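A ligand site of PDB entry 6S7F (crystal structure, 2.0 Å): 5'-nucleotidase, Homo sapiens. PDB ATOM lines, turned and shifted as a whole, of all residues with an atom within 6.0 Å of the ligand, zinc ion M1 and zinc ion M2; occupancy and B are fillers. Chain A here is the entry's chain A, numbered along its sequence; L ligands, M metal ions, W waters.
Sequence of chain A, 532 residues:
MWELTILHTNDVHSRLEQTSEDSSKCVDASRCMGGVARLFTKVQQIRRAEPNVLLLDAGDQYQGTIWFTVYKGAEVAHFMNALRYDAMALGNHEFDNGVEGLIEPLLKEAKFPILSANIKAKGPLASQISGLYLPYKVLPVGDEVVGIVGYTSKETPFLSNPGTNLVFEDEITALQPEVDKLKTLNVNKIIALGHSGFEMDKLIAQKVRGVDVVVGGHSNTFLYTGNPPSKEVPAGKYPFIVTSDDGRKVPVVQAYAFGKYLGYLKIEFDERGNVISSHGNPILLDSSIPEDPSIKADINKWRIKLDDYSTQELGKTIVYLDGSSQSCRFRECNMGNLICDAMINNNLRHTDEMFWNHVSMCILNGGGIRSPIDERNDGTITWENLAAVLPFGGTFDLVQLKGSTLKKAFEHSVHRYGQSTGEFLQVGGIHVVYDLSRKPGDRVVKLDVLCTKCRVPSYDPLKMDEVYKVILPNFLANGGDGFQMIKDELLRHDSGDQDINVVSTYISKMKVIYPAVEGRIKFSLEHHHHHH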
ATOM      1  N   ASP A  11      15.561  16.320 -26.789  1.00  0.00           N
ATOM      2  CA  ASP A  11      15.759  16.991 -25.507  1.00  0.00           C
ATOM      3  C   ASP A  11      16.895  18.026 -25.520  1.00  0.00           C
ATOM      4  O   ASP A  11      17.703  18.074 -24.599  1.00  0.00           O
ATOM      5  CB  ASP A  11      15.956  15.917 -24.413  1.00  0.00           C
ATOM      6  CG  ASP A  11      14.767  14.957 -24.338  1.00  0.00           C
ATOM      7  OD1 ASP A  11      14.749  13.967 -25.097  1.00  0.00           O
ATOM      8  OD2 ASP A  11      13.842  15.223 -23.546  1.00  0.00           O
ATOM      9  N   HIS A  13      16.620  21.210 -25.272  1.00  0.00           N
ATOM     10  CA  HIS A  13      16.344  22.085 -24.145  1.00  0.00           C
ATOM     11  C   HIS A  13      17.099  23.444 -24.210  1.00  0.00           C
ATOM     12  O   HIS A  13      17.806  23.841 -23.280  1.00  0.00           O
ATOM     13  CB  HIS A  13      16.573  21.311 -22.797  1.00  0.00           C
ATOM     14  CG  HIS A  13      15.475  20.348 -22.495  1.00  0.00           C
ATOM     15  ND1 HIS A  13      14.162  20.763 -22.426  1.00  0.00           N
ATOM     16  CD2 HIS A  13      15.508  19.006 -22.341  1.00  0.00           C
ATOM     17  CE1 HIS A  13      13.441  19.670 -22.245  1.00  0.00           C
ATOM     18  NE2 HIS A  13      14.210  18.582 -22.168  1.00  0.00           N
ATOM     19  N   GLY A  59      11.526  15.916 -29.930  1.00  0.00           N
ATOM     20  CA  GLY A  59      10.888  16.764 -28.946  1.00  0.00           C
ATOM     21  C   GLY A  59      11.785  17.336 -27.876  1.00  0.00           C
ATOM     22  O   GLY A  59      12.984  17.073 -27.812  1.00  0.00           O
ATOM     23  N   ASP A  60      11.173  18.182 -27.072  1.00  0.00           N
ATOM     24  CA  ASP A  60      11.764  18.910 -25.950  1.00  0.00           C
ATOM     25  C   ASP A  60      12.895  19.841 -26.383  1.00  0.00           C
ATOM     26  O   ASP A  60      13.980  19.834 -25.807  1.00  0.00           O
ATOM     27  CB  ASP A  60      12.164  17.928 -24.843  1.00  0.00           C
ATOM     28  CG  ASP A  60      11.120  17.599 -23.813  1.00  0.00           C
ATOM     29  OD1 ASP A  60       9.945  17.989 -23.995  1.00  0.00           O
ATOM     30  OD2 ASP A  60      11.449  16.846 -22.857  1.00  0.00           O
ATOM     31  N   GLN A  63      12.357  24.963 -23.363  1.00  0.00           N
ATOM     32  CA  GLN A  63      12.753  25.021 -21.965  1.00  0.00           C
ATOM     33  C   GLN A  63      14.180  24.554 -21.630  1.00  0.00           C
ATOM     34  O   GLN A  63      14.505  23.399 -21.852  1.00  0.00           O
ATOM     35  CB  GLN A  63      11.738  24.239 -21.106  1.00  0.00           C
ATOM     36  CG  GLN A  63      11.549  24.762 -19.705  1.00  0.00           C
ATOM     37  CD  GLN A  63      10.866  26.110 -19.661  1.00  0.00           C
ATOM     38  OE1 GLN A  63      11.524  27.149 -19.633  1.00  0.00           O
ATOM     39  NE2 GLN A  63       9.552  26.117 -19.532  1.00  0.00           N
ATOM     40  N   GLY A  91       7.089  17.312 -27.991  1.00  0.00           N
ATOM     41  CA  GLY A  91       7.487  16.827 -26.665  1.00  0.00           C
ATOM     42  C   GLY A  91       6.625  17.498 -25.618  1.00  0.00           C
ATOM     43  O   GLY A  91       5.824  18.368 -25.948  1.00  0.00           O
ATOM     44  N   ASN A  92       6.784  17.105 -24.345  1.00  0.00           N
ATOM     45  CA  ASN A  92       5.955  17.656 -23.283  1.00  0.00           C
ATOM     46  C   ASN A  92       6.292  19.119 -22.997  1.00  0.00           C
ATOM     47  O   ASN A  92       5.363  19.905 -22.770  1.00  0.00           O
ATOM     48  CB  ASN A  92       5.954  16.807 -22.000  1.00  0.00           C
ATOM     49  CG  ASN A  92       7.299  16.342 -21.521  1.00  0.00           C
ATOM     50  OD1 ASN A  92       7.968  15.551 -22.190  1.00  0.00           O
ATOM     51  ND2 ASN A  92       7.775  16.874 -20.428  1.00  0.00           N
ATOM     52  N   HIS A  93       7.586  19.511 -23.047  1.00  0.00           N
ATOM     53  CA  HIS A  93       7.962  20.908 -22.780  1.00  0.00           C
ATOM     54  C   HIS A  93       7.559  21.873 -23.914  1.00  0.00           C
ATOM     55  O   HIS A  93       7.564  23.078 -23.706  1.00  0.00           O
ATOM     56  CB  HIS A  93       9.451  21.035 -22.426  1.00  0.00           C
ATOM     57  CG  HIS A  93       9.761  20.451 -21.073  1.00  0.00           C
ATOM     58  ND1 HIS A  93       9.560  21.161 -19.915  1.00  0.00           N
ATOM     59  CD2 HIS A  93      10.201  19.218 -20.740  1.00  0.00           C
ATOM     60  CE1 HIS A  93       9.843  20.332 -18.924  1.00  0.00           C
ATOM     61  NE2 HIS A  93      10.281  19.176 -19.369  1.00  0.00           N
ATOM     62  N   PHE A  95       4.579  22.389 -24.628  1.00  0.00           N
ATOM     63  CA  PHE A  95       3.332  22.930 -24.059  1.00  0.00           C
ATOM     64  C   PHE A  95       3.544  23.722 -22.747  1.00  0.00           C
ATOM     65  O   PHE A  95       2.551  24.025 -22.089  1.00  0.00           O
ATOM     66  CB  PHE A  95       2.351  21.768 -23.785  1.00  0.00           C
ATOM     67  CG  PHE A  95       1.978  20.980 -25.014  1.00  0.00           C
ATOM     68  CD1 PHE A  95       0.885  21.347 -25.804  1.00  0.00           C
ATOM     69  CD2 PHE A  95       2.745  19.888 -25.414  1.00  0.00           C
ATOM     70  CE1 PHE A  95       0.555  20.624 -26.941  1.00  0.00           C
ATOM     71  CE2 PHE A  95       2.439  19.197 -26.593  1.00  0.00           C
ATOM     72  CZ  PHE A  95       1.361  19.573 -27.346  1.00  0.00           C
ATOM     73  N   ASP A  96       4.798  24.041 -22.336  1.00  0.00           N
ATOM     74  CA  ASP A  96       5.044  24.742 -21.068  1.00  0.00           C
ATOM     75  C   ASP A  96       4.417  26.140 -20.992  1.00  0.00           C
ATOM     76  O   ASP A  96       4.027  26.583 -19.888  1.00  0.00           O
ATOM     77  CB  ASP A  96       6.548  24.828 -20.758  1.00  0.00           C
ATOM     78  CG  ASP A  96       7.181  23.559 -20.181  1.00  0.00           C
ATOM     79  OD1 ASP A  96       6.486  22.522 -20.111  1.00  0.00           O
ATOM     80  OD2 ASP A  96       8.358  23.606 -19.818  1.00  0.00           O
ATOM     81  N   ASN A  97       4.294  26.822 -22.144  1.00  0.00           N
ATOM     82  CA  ASN A  97       3.685  28.150 -22.230  1.00  0.00           C
ATOM     83  C   ASN A  97       2.284  28.026 -22.836  1.00  0.00           C
ATOM     84  O   ASN A  97       1.809  28.944 -23.522  1.00  0.00           O
ATOM     85  CB  ASN A  97       4.594  29.073 -23.048  1.00  0.00           C
ATOM     86  CG  ASN A  97       5.870  29.388 -22.317  1.00  0.00           C
ATOM     87  OD1 ASN A  97       5.971  29.237 -21.098  1.00  0.00           O
ATOM     88  ND2 ASN A  97       6.882  29.840 -23.052  1.00  0.00           N
ATOM     89  N   LEU A 159       2.604  16.679 -16.810  1.00  0.00           N
ATOM     90  CA  LEU A 159       3.963  17.229 -16.898  1.00  0.00           C
ATOM     91  C   LEU A 159       4.061  18.685 -17.358  1.00  0.00           C
ATOM     92  O   LEU A 159       5.044  19.370 -17.014  1.00  0.00           O
ATOM     93  CB  LEU A 159       4.787  16.374 -17.852  1.00  0.00           C
ATOM     94  CG  LEU A 159       4.968  14.913 -17.490  1.00  0.00           C
ATOM     95  CD1 LEU A 159       5.455  14.138 -18.701  1.00  0.00           C
ATOM     96  CD2 LEU A 159       5.837  14.739 -16.262  1.00  0.00           C
ATOM     97  N   SER A 160       3.098  19.147 -18.157  1.00  0.00           N
ATOM     98  CA  SER A 160       3.121  20.501 -18.727  1.00  0.00           C
ATOM     99  C   SER A 160       1.762  21.210 -18.549  1.00  0.00           C
ATOM    100  O   SER A 160       1.055  20.974 -17.566  1.00  0.00           O
ATOM    101  CB  SER A 160       3.523  20.391 -20.197  1.00  0.00           C
ATOM    102  OG  SER A 160       4.010  21.616 -20.692  1.00  0.00           O
ATOM    103  N   ASN A 161       1.423  22.119 -19.500  1.00  0.00           N
ATOM    104  CA  ASN A 161       0.158  22.854 -19.518  1.00  0.00           C
ATOM    105  C   ASN A 161      -0.490  22.776 -20.920  1.00  0.00           C
ATOM    106  O   ASN A 161      -0.746  23.799 -21.547  1.00  0.00           O
ATOM    107  CB  ASN A 161       0.409  24.316 -19.054  1.00  0.00           C
ATOM    108  CG  ASN A 161      -0.811  25.060 -18.581  1.00  0.00           C
ATOM    109  OD1 ASN A 161      -1.926  24.535 -18.552  1.00  0.00           O
ATOM    110  ND2 ASN A 161      -0.611  26.316 -18.193  1.00  0.00           N
ATOM    111  N   HIS A 195       8.097  11.370 -28.457  1.00  0.00           N
ATOM    112  CA  HIS A 195       8.568  11.824 -27.177  1.00  0.00           C
ATOM    113  C   HIS A 195       7.849  11.206 -25.983  1.00  0.00           C
ATOM    114  O   HIS A 195       7.043  11.849 -25.352  1.00  0.00           O
ATOM    115  CB  HIS A 195       8.445  13.357 -27.170  1.00  0.00           C
ATOM    116  CG  HIS A 195       9.282  13.979 -26.095  1.00  0.00           C
ATOM    117  ND1 HIS A 195      10.610  14.187 -26.270  1.00  0.00           N
ATOM    118  CD2 HIS A 195       8.965  14.239 -24.820  1.00  0.00           C
ATOM    119  CE1 HIS A 195      11.061  14.646 -25.135  1.00  0.00           C
ATOM    120  NE2 HIS A 195      10.112  14.671 -24.227  1.00  0.00           N
ATOM    121  N   GLY A 217      12.892  10.063 -27.524  1.00  0.00           N
ATOM    122  CA  GLY A 217      13.417  11.060 -26.595  1.00  0.00           C
ATOM    123  C   GLY A 217      12.799  10.867 -25.240  1.00  0.00           C
ATOM    124  O   GLY A 217      12.363   9.765 -24.886  1.00  0.00           O
ATOM    125  N   HIS A 218      12.789  11.954 -24.461  1.00  0.00           N
ATOM    126  CA  HIS A 218      12.141  12.103 -23.176  1.00  0.00           C
ATOM    127  C   HIS A 218      12.926  11.498 -21.975  1.00  0.00           C
ATOM    128  O   HIS A 218      12.951  12.145 -20.934  1.00  0.00           O
ATOM    129  CB  HIS A 218      10.713  11.590 -23.224  1.00  0.00           C
ATOM    130  CG  HIS A 218       9.905  11.923 -22.006  1.00  0.00           C
ATOM    131  ND1 HIS A 218       9.757  13.217 -21.582  1.00  0.00           N
ATOM    132  CD2 HIS A 218       9.250  11.105 -21.175  1.00  0.00           C
ATOM    133  CE1 HIS A 218       8.991  13.145 -20.508  1.00  0.00           C
ATOM    134  NE2 HIS A 218       8.689  11.888 -20.216  1.00  0.00           N
ATOM    135  N   SER A 219      13.566  10.323 -22.108  1.00  0.00           N
ATOM    136  CA  SER A 219      14.334   9.705 -21.036  1.00  0.00           C
ATOM    137  C   SER A 219      15.852  10.028 -21.067  1.00  0.00           C
ATOM    138  O   SER A 219      16.620   9.539 -20.225  1.00  0.00           O
ATOM    139  CB  SER A 219      14.085   8.194 -21.031  1.00  0.00           C
ATOM    140  OG  SER A 219      14.198   7.654 -22.324  1.00  0.00           O
ATOM    141  N   ASN A 220      16.273  10.906 -21.997  1.00  0.00           N
ATOM    142  CA  ASN A 220      17.679  11.308 -22.189  1.00  0.00           C
ATOM    143  C   ASN A 220      18.593  10.083 -22.314  1.00  0.00           C
ATOM    144  O   ASN A 220      19.696  10.076 -21.824  1.00  0.00           O
ATOM    145  CB  ASN A 220      18.120  12.262 -21.051  1.00  0.00           C
ATOM    146  CG  ASN A 220      17.141  13.403 -20.885  1.00  0.00           C
ATOM    147  OD1 ASN A 220      16.451  13.806 -21.830  1.00  0.00           O
ATOM    148  ND2 ASN A 220      17.073  13.996 -19.715  1.00  0.00           N
ATOM    149  N   ARG A 329      19.618  12.850  -8.998  1.00  0.00           N
ATOM    150  CA  ARG A 329      18.544  11.854  -9.045  1.00  0.00           C
ATOM    151  C   ARG A 329      19.001  10.568  -8.430  1.00  0.00           C
ATOM    152  O   ARG A 329      18.267   9.568  -8.499  1.00  0.00           O
ATOM    153  CB  ARG A 329      18.082  11.629 -10.486  1.00  0.00           C
ATOM    154  CG  ARG A 329      17.653  12.881 -11.200  1.00  0.00           C
ATOM    155  CD  ARG A 329      17.129  12.566 -12.580  1.00  0.00           C
ATOM    156  NE  ARG A 329      16.801  13.792 -13.290  1.00  0.00           N
ATOM    157  CZ  ARG A 329      15.923  13.910 -14.285  1.00  0.00           C
ATOM    158  NH1 ARG A 329      15.252  12.852 -14.722  1.00  0.00           N
ATOM    159  NH2 ARG A 329      15.715  15.092 -14.854  1.00  0.00           N
ATOM    160  N   ASN A 365      12.370  18.122  -5.612  1.00  0.00           N
ATOM    161  CA  ASN A 365      12.553  17.060  -6.607  1.00  0.00           C
ATOM    162  C   ASN A 365      13.875  17.279  -7.365  1.00  0.00           C
ATOM    163  O   ASN A 365      14.064  18.319  -7.982  1.00  0.00           O
ATOM    164  CB  ASN A 365      11.357  17.002  -7.641  1.00  0.00           C
ATOM    165  CG  ASN A 365      10.991  18.342  -8.260  1.00  0.00           C
ATOM    166  OD1 ASN A 365      10.708  19.317  -7.562  1.00  0.00           O
ATOM    167  ND2 ASN A 365      11.072  18.469  -9.559  1.00  0.00           N
ATOM    168  N   GLY A 366      14.745  16.271  -7.353  1.00  0.00           N
ATOM    169  CA  GLY A 366      16.010  16.267  -8.089  1.00  0.00           C
ATOM    170  C   GLY A 366      15.893  16.608  -9.583  1.00  0.00           C
ATOM    171  O   GLY A 366      16.796  17.222 -10.146  1.00  0.00           O
ATOM    172  N   GLY A 367      14.781  16.208 -10.220  1.00  0.00           N
ATOM    173  CA  GLY A 367      14.536  16.516 -11.615  1.00  0.00           C
ATOM    174  C   GLY A 367      14.310  17.996 -11.935  1.00  0.00           C
ATOM    175  O   GLY A 367      14.490  18.421 -13.083  1.00  0.00           O
ATOM    176  N   GLY A 368      13.886  18.774 -10.930  1.00  0.00           N
ATOM    177  CA  GLY A 368      13.694  20.207 -11.066  1.00  0.00           C
ATOM    178  C   GLY A 368      14.991  21.000 -11.164  1.00  0.00           C
ATOM    179  O   GLY A 368      14.956  22.197 -11.490  1.00  0.00           O
ATOM    180  N   ARG A 370      17.795  21.559 -13.221  1.00  0.00           N
ATOM    181  CA  ARG A 370      17.951  21.277 -14.646  1.00  0.00           C
ATOM    182  C   ARG A 370      19.339  21.496 -15.206  1.00  0.00           C
ATOM    183  O   ARG A 370      19.567  21.213 -16.391  1.00  0.00           O
ATOM    184  CB  ARG A 370      16.927  22.087 -15.442  1.00  0.00           C
ATOM    185  CG  ARG A 370      15.470  21.771 -15.098  1.00  0.00           C
ATOM    186  CD  ARG A 370      15.013  20.375 -15.521  1.00  0.00           C
ATOM    187  NE  ARG A 370      14.694  20.261 -16.947  1.00  0.00           N
ATOM    188  CZ  ARG A 370      14.065  19.224 -17.519  1.00  0.00           C
ATOM    189  NH1 ARG A 370      13.813  19.226 -18.817  1.00  0.00           N
ATOM    190  NH2 ARG A 370      13.660  18.186 -16.780  1.00  0.00           N
ATOM    191  N   PHE A 392      11.654  26.740 -14.976  1.00  0.00           N
ATOM    192  CA  PHE A 392      10.202  26.600 -15.052  1.00  0.00           C
ATOM    193  C   PHE A 392       9.348  27.711 -14.479  1.00  0.00           C
ATOM    194  O   PHE A 392       8.131  27.627 -14.610  1.00  0.00           O
ATOM    195  CB  PHE A 392       9.768  25.276 -14.383  1.00  0.00           C
ATOM    196  CG  PHE A 392      10.455  24.044 -14.924  1.00  0.00           C
ATOM    197  CD1 PHE A 392      10.439  23.763 -16.275  1.00  0.00           C
ATOM    198  CD2 PHE A 392      11.151  23.199 -14.098  1.00  0.00           C
ATOM    199  CE1 PHE A 392      11.141  22.674 -16.781  1.00  0.00           C
ATOM    200  CE2 PHE A 392      11.813  22.078 -14.601  1.00  0.00           C
ATOM    201  CZ  PHE A 392      11.798  21.822 -15.938  1.00  0.00           C
ATOM    202  N   SER A 420      17.109   7.054 -12.956  1.00  0.00           N
ATOM    203  CA  SER A 420      17.321   8.496 -13.240  1.00  0.00           C
ATOM    204  C   SER A 420      15.967   9.253 -13.324  1.00  0.00           C
ATOM    205  O   SER A 420      15.736  10.055 -14.222  1.00  0.00           O
ATOM    206  CB  SER A 420      18.142   8.718 -14.505  1.00  0.00           C
ATOM    207  OG  SER A 420      18.744  10.004 -14.511  1.00  0.00           O
ATOM    208  N   THR A 421      15.073   8.981 -12.380  1.00  0.00           N
ATOM    209  CA  THR A 421      13.765   9.624 -12.348  1.00  0.00           C
ATOM    210  C   THR A 421      13.877  10.837 -11.408  1.00  0.00           C
ATOM    211  O   THR A 421      14.622  10.816 -10.421  1.00  0.00           O
ATOM    212  CB  THR A 421      12.666   8.588 -12.049  1.00  0.00           C
ATOM    213  OG1 THR A 421      12.916   7.950 -10.779  1.00  0.00           O
ATOM    214  CG2 THR A 421      12.544   7.553 -13.145  1.00  0.00           C
ATOM    215  N   GLY A 422      13.172  11.899 -11.768  1.00  0.00           N
ATOM    216  CA  GLY A 422      13.261  13.164 -11.078  1.00  0.00           C
ATOM    217  C   GLY A 422      12.655  13.274  -9.706  1.00  0.00           C
ATOM    218  O   GLY A 422      12.902  14.269  -9.041  1.00  0.00           O
ATOM    219  N   GLU A 423      11.900  12.267  -9.251  1.00  0.00           N
ATOM    220  CA  GLU A 423      11.274  12.297  -7.950  1.00  0.00           C
ATOM    221  C   GLU A 423      12.258  12.138  -6.762  1.00  0.00           C
ATOM    222  O   GLU A 423      11.819  12.312  -5.656  1.00  0.00           O
ATOM    223  CB  GLU A 423      10.135  11.284  -7.807  1.00  0.00           C
ATOM    224  CG  GLU A 423      10.555   9.829  -7.623  1.00  0.00           C
ATOM    225  CD  GLU A 423      10.770   9.078  -8.908  1.00  0.00           C
ATOM    226  OE1 GLU A 423      10.755   7.827  -8.885  1.00  0.00           O
ATOM    227  OE2 GLU A 423      10.943   9.743  -9.960  1.00  0.00           O
ATOM    228  N   PHE A 475       5.364  22.555  -7.814  1.00  0.00           N
ATOM    229  CA  PHE A 475       5.311  21.337  -8.615  1.00  0.00           C
ATOM    230  C   PHE A 475       5.038  20.127  -7.715  1.00  0.00           C
ATOM    231  O   PHE A 475       4.178  19.314  -8.054  1.00  0.00           O
ATOM    232  CB  PHE A 475       6.616  21.171  -9.431  1.00  0.00           C
ATOM    233  CG  PHE A 475       6.775  19.846 -10.149  1.00  0.00           C
ATOM    234  CD1 PHE A 475       6.068  19.579 -11.309  1.00  0.00           C
ATOM    235  CD2 PHE A 475       7.592  18.847  -9.633  1.00  0.00           C
ATOM    236  CE1 PHE A 475       6.151  18.329 -11.922  1.00  0.00           C
ATOM    237  CE2 PHE A 475       7.703  17.626 -10.257  1.00  0.00           C
ATOM    238  CZ  PHE A 475       6.987  17.371 -11.408  1.00  0.00           C
ATOM    239  N   ASP A 481       5.452  14.628 -10.157  1.00  0.00           N
ATOM    240  CA  ASP A 481       6.364  13.486  -9.981  1.00  0.00           C
ATOM    241  C   ASP A 481       5.758  12.358  -9.163  1.00  0.00           C
ATOM    242  O   ASP A 481       6.469  11.661  -8.448  1.00  0.00           O
ATOM    243  CB  ASP A 481       7.732  13.945  -9.393  1.00  0.00           C
ATOM    244  CG  ASP A 481       8.827  14.194 -10.420  1.00  0.00           C
ATOM    245  OD1 ASP A 481       8.718  13.704 -11.561  1.00  0.00           O
ATOM    246  OD2 ASP A 481       9.844  14.815 -10.044  1.00  0.00           O
HETATM  247  N1  LIG L   1       8.511  21.712 -12.569  1.00  0.00           N
HETATM  248  N2  LIG L   1       9.993  19.851 -12.215  1.00  0.00           N
HETATM  249  C1  LIG L   1       9.744  19.538 -13.497  1.00  0.00           C
HETATM  250  C2  LIG L   1       8.912  20.213 -14.366  1.00  0.00           C
HETATM  251  C3  LIG L   1       8.272  21.370 -13.844  1.00  0.00           C
HETATM  252  C4  LIG L   1       9.767  18.621 -15.473  1.00  0.00           C
HETATM  253  C5  LIG L   1       7.049  21.963 -15.920  1.00  0.00           C
HETATM  254  C6  LIG L   1       3.720  24.507 -16.887  1.00  0.00           C
HETATM  255  C7  LIG L   1       6.079  24.079 -16.903  1.00  0.00           C
HETATM  256  C8  LIG L   1       4.589  22.491 -15.905  1.00  0.00           C
HETATM  257  P1  LIG L   1      11.642  16.091 -19.493  1.00  0.00           P
HETATM  258  O1  LIG L   1      12.746  16.868 -20.134  1.00  0.00           O
HETATM  259  O2  LIG L   1      10.421  15.927 -20.414  1.00  0.00           O
HETATM  260  O3  LIG L   1      11.105  16.876 -18.279  1.00  0.00           O
HETATM  261  P2  LIG L   1      13.710  14.533 -17.901  1.00  0.00           P
HETATM  262  O4  LIG L   1      14.957  15.239 -18.303  1.00  0.00           O
HETATM  263  O5  LIG L   1      13.994  13.077 -17.449  1.00  0.00           O
HETATM  264  C9  LIG L   1      12.206  14.492 -18.908  1.00  0.00           C
HETATM  265  O6  LIG L   1      13.202  15.294 -16.621  1.00  0.00           O
HETATM  266  C10 LIG L   1      12.061  14.832 -15.867  1.00  0.00           C
HETATM  267  C11 LIG L   1      11.994  15.518 -14.533  1.00  0.00           C
HETATM  268  O7  LIG L   1      11.957  16.944 -14.719  1.00  0.00           O
HETATM  269  C12 LIG L   1      10.723  15.196 -13.777  1.00  0.00           C
HETATM  270  O8  LIG L   1      10.887  13.922 -13.158  1.00  0.00           O
HETATM  271  C13 LIG L   1      10.580  16.397 -12.853  1.00  0.00           C
HETATM  272  O9  LIG L   1      11.324  16.242 -11.655  1.00  0.00           O
HETATM  273  C14 LIG L   1      11.218  17.528 -13.666  1.00  0.00           C
HETATM  274  N3  LIG L   1      10.286  18.505 -14.214  1.00  0.00           N
HETATM  275  N4  LIG L   1       8.930  19.619 -15.613  1.00  0.00           N
HETATM  276  N5  LIG L   1       7.434  22.162 -14.534  1.00  0.00           N
HETATM  277  C15 LIG L   1       9.333  20.948 -11.852  1.00  0.00           C
HETATM  278  C16 LIG L   1       5.008  24.893 -17.215  1.00  0.00           C
HETATM  279  C17 LIG L   1       5.883  22.859 -16.261  1.00  0.00           C
HETATM  280  C18 LIG L   1       3.516  23.300 -16.236  1.00  0.00           C
HETATM  281 ZN    ZN M   1      13.574  16.696 -22.039  1.00  0.00          ZN
HETATM  282 ZN    ZN M   2      10.043  15.203 -22.220  1.00  0.00          ZN
HETATM  283  O   HOH W   1      10.780  21.559  -9.057  1.00  0.00           O
HETATM  284  O   HOH W   2       7.100  24.125 -12.072  1.00  0.00           O
HETATM  285  O   HOH W   3       8.613  15.631 -17.380  1.00  0.00           O
HETATM  286  O   HOH W   4      15.850  11.206 -17.860  1.00  0.00           O
HETATM  287  O   HOH W   5      12.071  11.231 -17.068  1.00  0.00           O
HETATM  288  O   HOH W   6      11.233  11.349 -14.161  1.00  0.00           O
HETATM  289  O   HOH W   7      15.142  16.126 -21.095  1.00  0.00           O
HETATM  290  O   HOH W   8      17.090  16.945 -17.483  1.00  0.00           O
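NE2 of His 93 is in hydrogen-bond range of O3 of the ligand (2.7 Å). The side-chain amide nitrogen (ND2) of Asn 220 is in hydrogen-bond range of an oxygen (O4) of the ligand (2.8 Å). The backbone NH (N) of Gly 422 lies close to an oxygen (O8) of the ligand (3.4 Å). OD2 of Asp 481 lies within hydrogen-bond range of O9 of the ligand (2.6 Å). ND2 of Asn 365 sits at hydrogen-bond distance from O9 of the ligand (3.1 Å). The guanidinium group (NH2) of Arg 370 lies within salt-bridge range of an oxygen (O3) of the ligand (3.2 Å). NH1 of Arg 329 is in salt-bridge range of O5 of the ligand (3.0 Å).
The side-chain hydroxyl (OG) of Ser 160 is in hydrogen-bond range of the side-chain carboxylate (OD1) of Asp 96 (2.7 Å). The side-chain amide nitrogen (NE2) of Gln 63 lies within hydrogen-bond range of the side-chain carboxylate (OD2) of Asp 96 (2.8 Å). A ring nitrogen (ND1) of His 13 lies within hydrogen-bond range of the backbone carbonyl oxygen (O) of Gln 63 (2.7 Å). The side-chain hydroxyl of Ser 160 sits close to the backbone carbonyl oxygen of Phe 95. The side-chain carboxylate of Asp 96 is in hydrogen-bond range of a ring nitrogen (ND1) of His 93 (2.7 Å). The backbone carbonyl oxygen of Ser 420 lies within hydrogen-bond range of the guanidinium group of Arg 329. N of His 93 lies within hydrogen-bond range of OD1 of Asp 60, at 3.0 Å. The backbone carbonyl oxygen of Asn 92 sits at hydrogen-bond distance from the side-chain hydroxyl of Ser 160 (3.0 Å).
The backbone carbonyl oxygen of Gly 367 lies close to an oxygen (O7) of the ligand (3.4 Å). Asp 96 touches the ligand (O to C16, 3.3 Å). Leu 159 touches the ligand. Ser 160 touches the ligand. Asn 161 touches the ligand. N of Gly 368 touches O9 of the ligand, 3.7 Å away. Phe 392 touches the ligand (CD2 to N1, 3.4 Å). Phe 475 touches the ligand (CG to C15, 3.3 Å). Within 4 Å of the ligand: Asp 11, His 13, Asp 60, Asn 92, His 93, Asp 96, Leu 159, Ser 160, Asn 161, His 218, Asn 220, Arg 329, Asn 365, Gly 367, Gly 368, Arg 370, Phe 392, Gly 422, Phe 475 and Asp 481. The nearest printed residue that does not touch the ligand is His 195 (4.03 Å).
Within 4 Å of zinc ion M1: Asp 11, His 13 and Asp 60.
Within 4 Å of zinc ion M2: Asp 60, Asn 92, His 195 and His 218. The nearest printed residue that does not touch zinc ion M2 is Asp 11 (4.02 Å).
Water W7 binds zinc ion M1 (1.9 Å). Zinc ion M1 is bound by NE2 of His 13, 2.0 Å away. Zinc ion M1 is bound by an oxygen (O1) of the ligand (2.1 Å). OD2 of Asp 11 binds zinc ion M1, at 2.1 Å. OD2 of Asp 60 binds zinc ion M1.
Zinc ion M2 is bound by an oxygen (O2) of the ligand, at 2.0 Å. Zinc ion M2 is bound by a ring nitrogen (NE2) of His 195 (2.1 Å). Zinc ion M2 is bound by OD1 of Asn 92 (2.1 Å). Zinc ion M2 is bound by ND1 of His 218 (2.1 Å). Zinc ion M2 is bound by OD2 of Asp 60, 2.3 Å away. Zinc ion M2 has five donor atoms within binding distance.
Water W7 lies within hydrogen-bond range of OD1 of Asn 220 (2.8 Å) and O4 of the ligand (2.9 Å). Water W4 lies within hydrogen-bond range of an oxygen (O5) of the ligand and the backbone carbonyl oxygen of Ser 219. Water W6 bridges O8 of the ligand (2.8 Å) and N of Gly 422 (3.1 Å). Water W8 lies within hydrogen-bond range of O4 of the ligand (2.9 Å) and NH2 of Arg 329 (3.5 Å). Water W3 bridges O3 of the ligand (2.9 Å) and ND2 of Asn 92 (3.4 Å).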
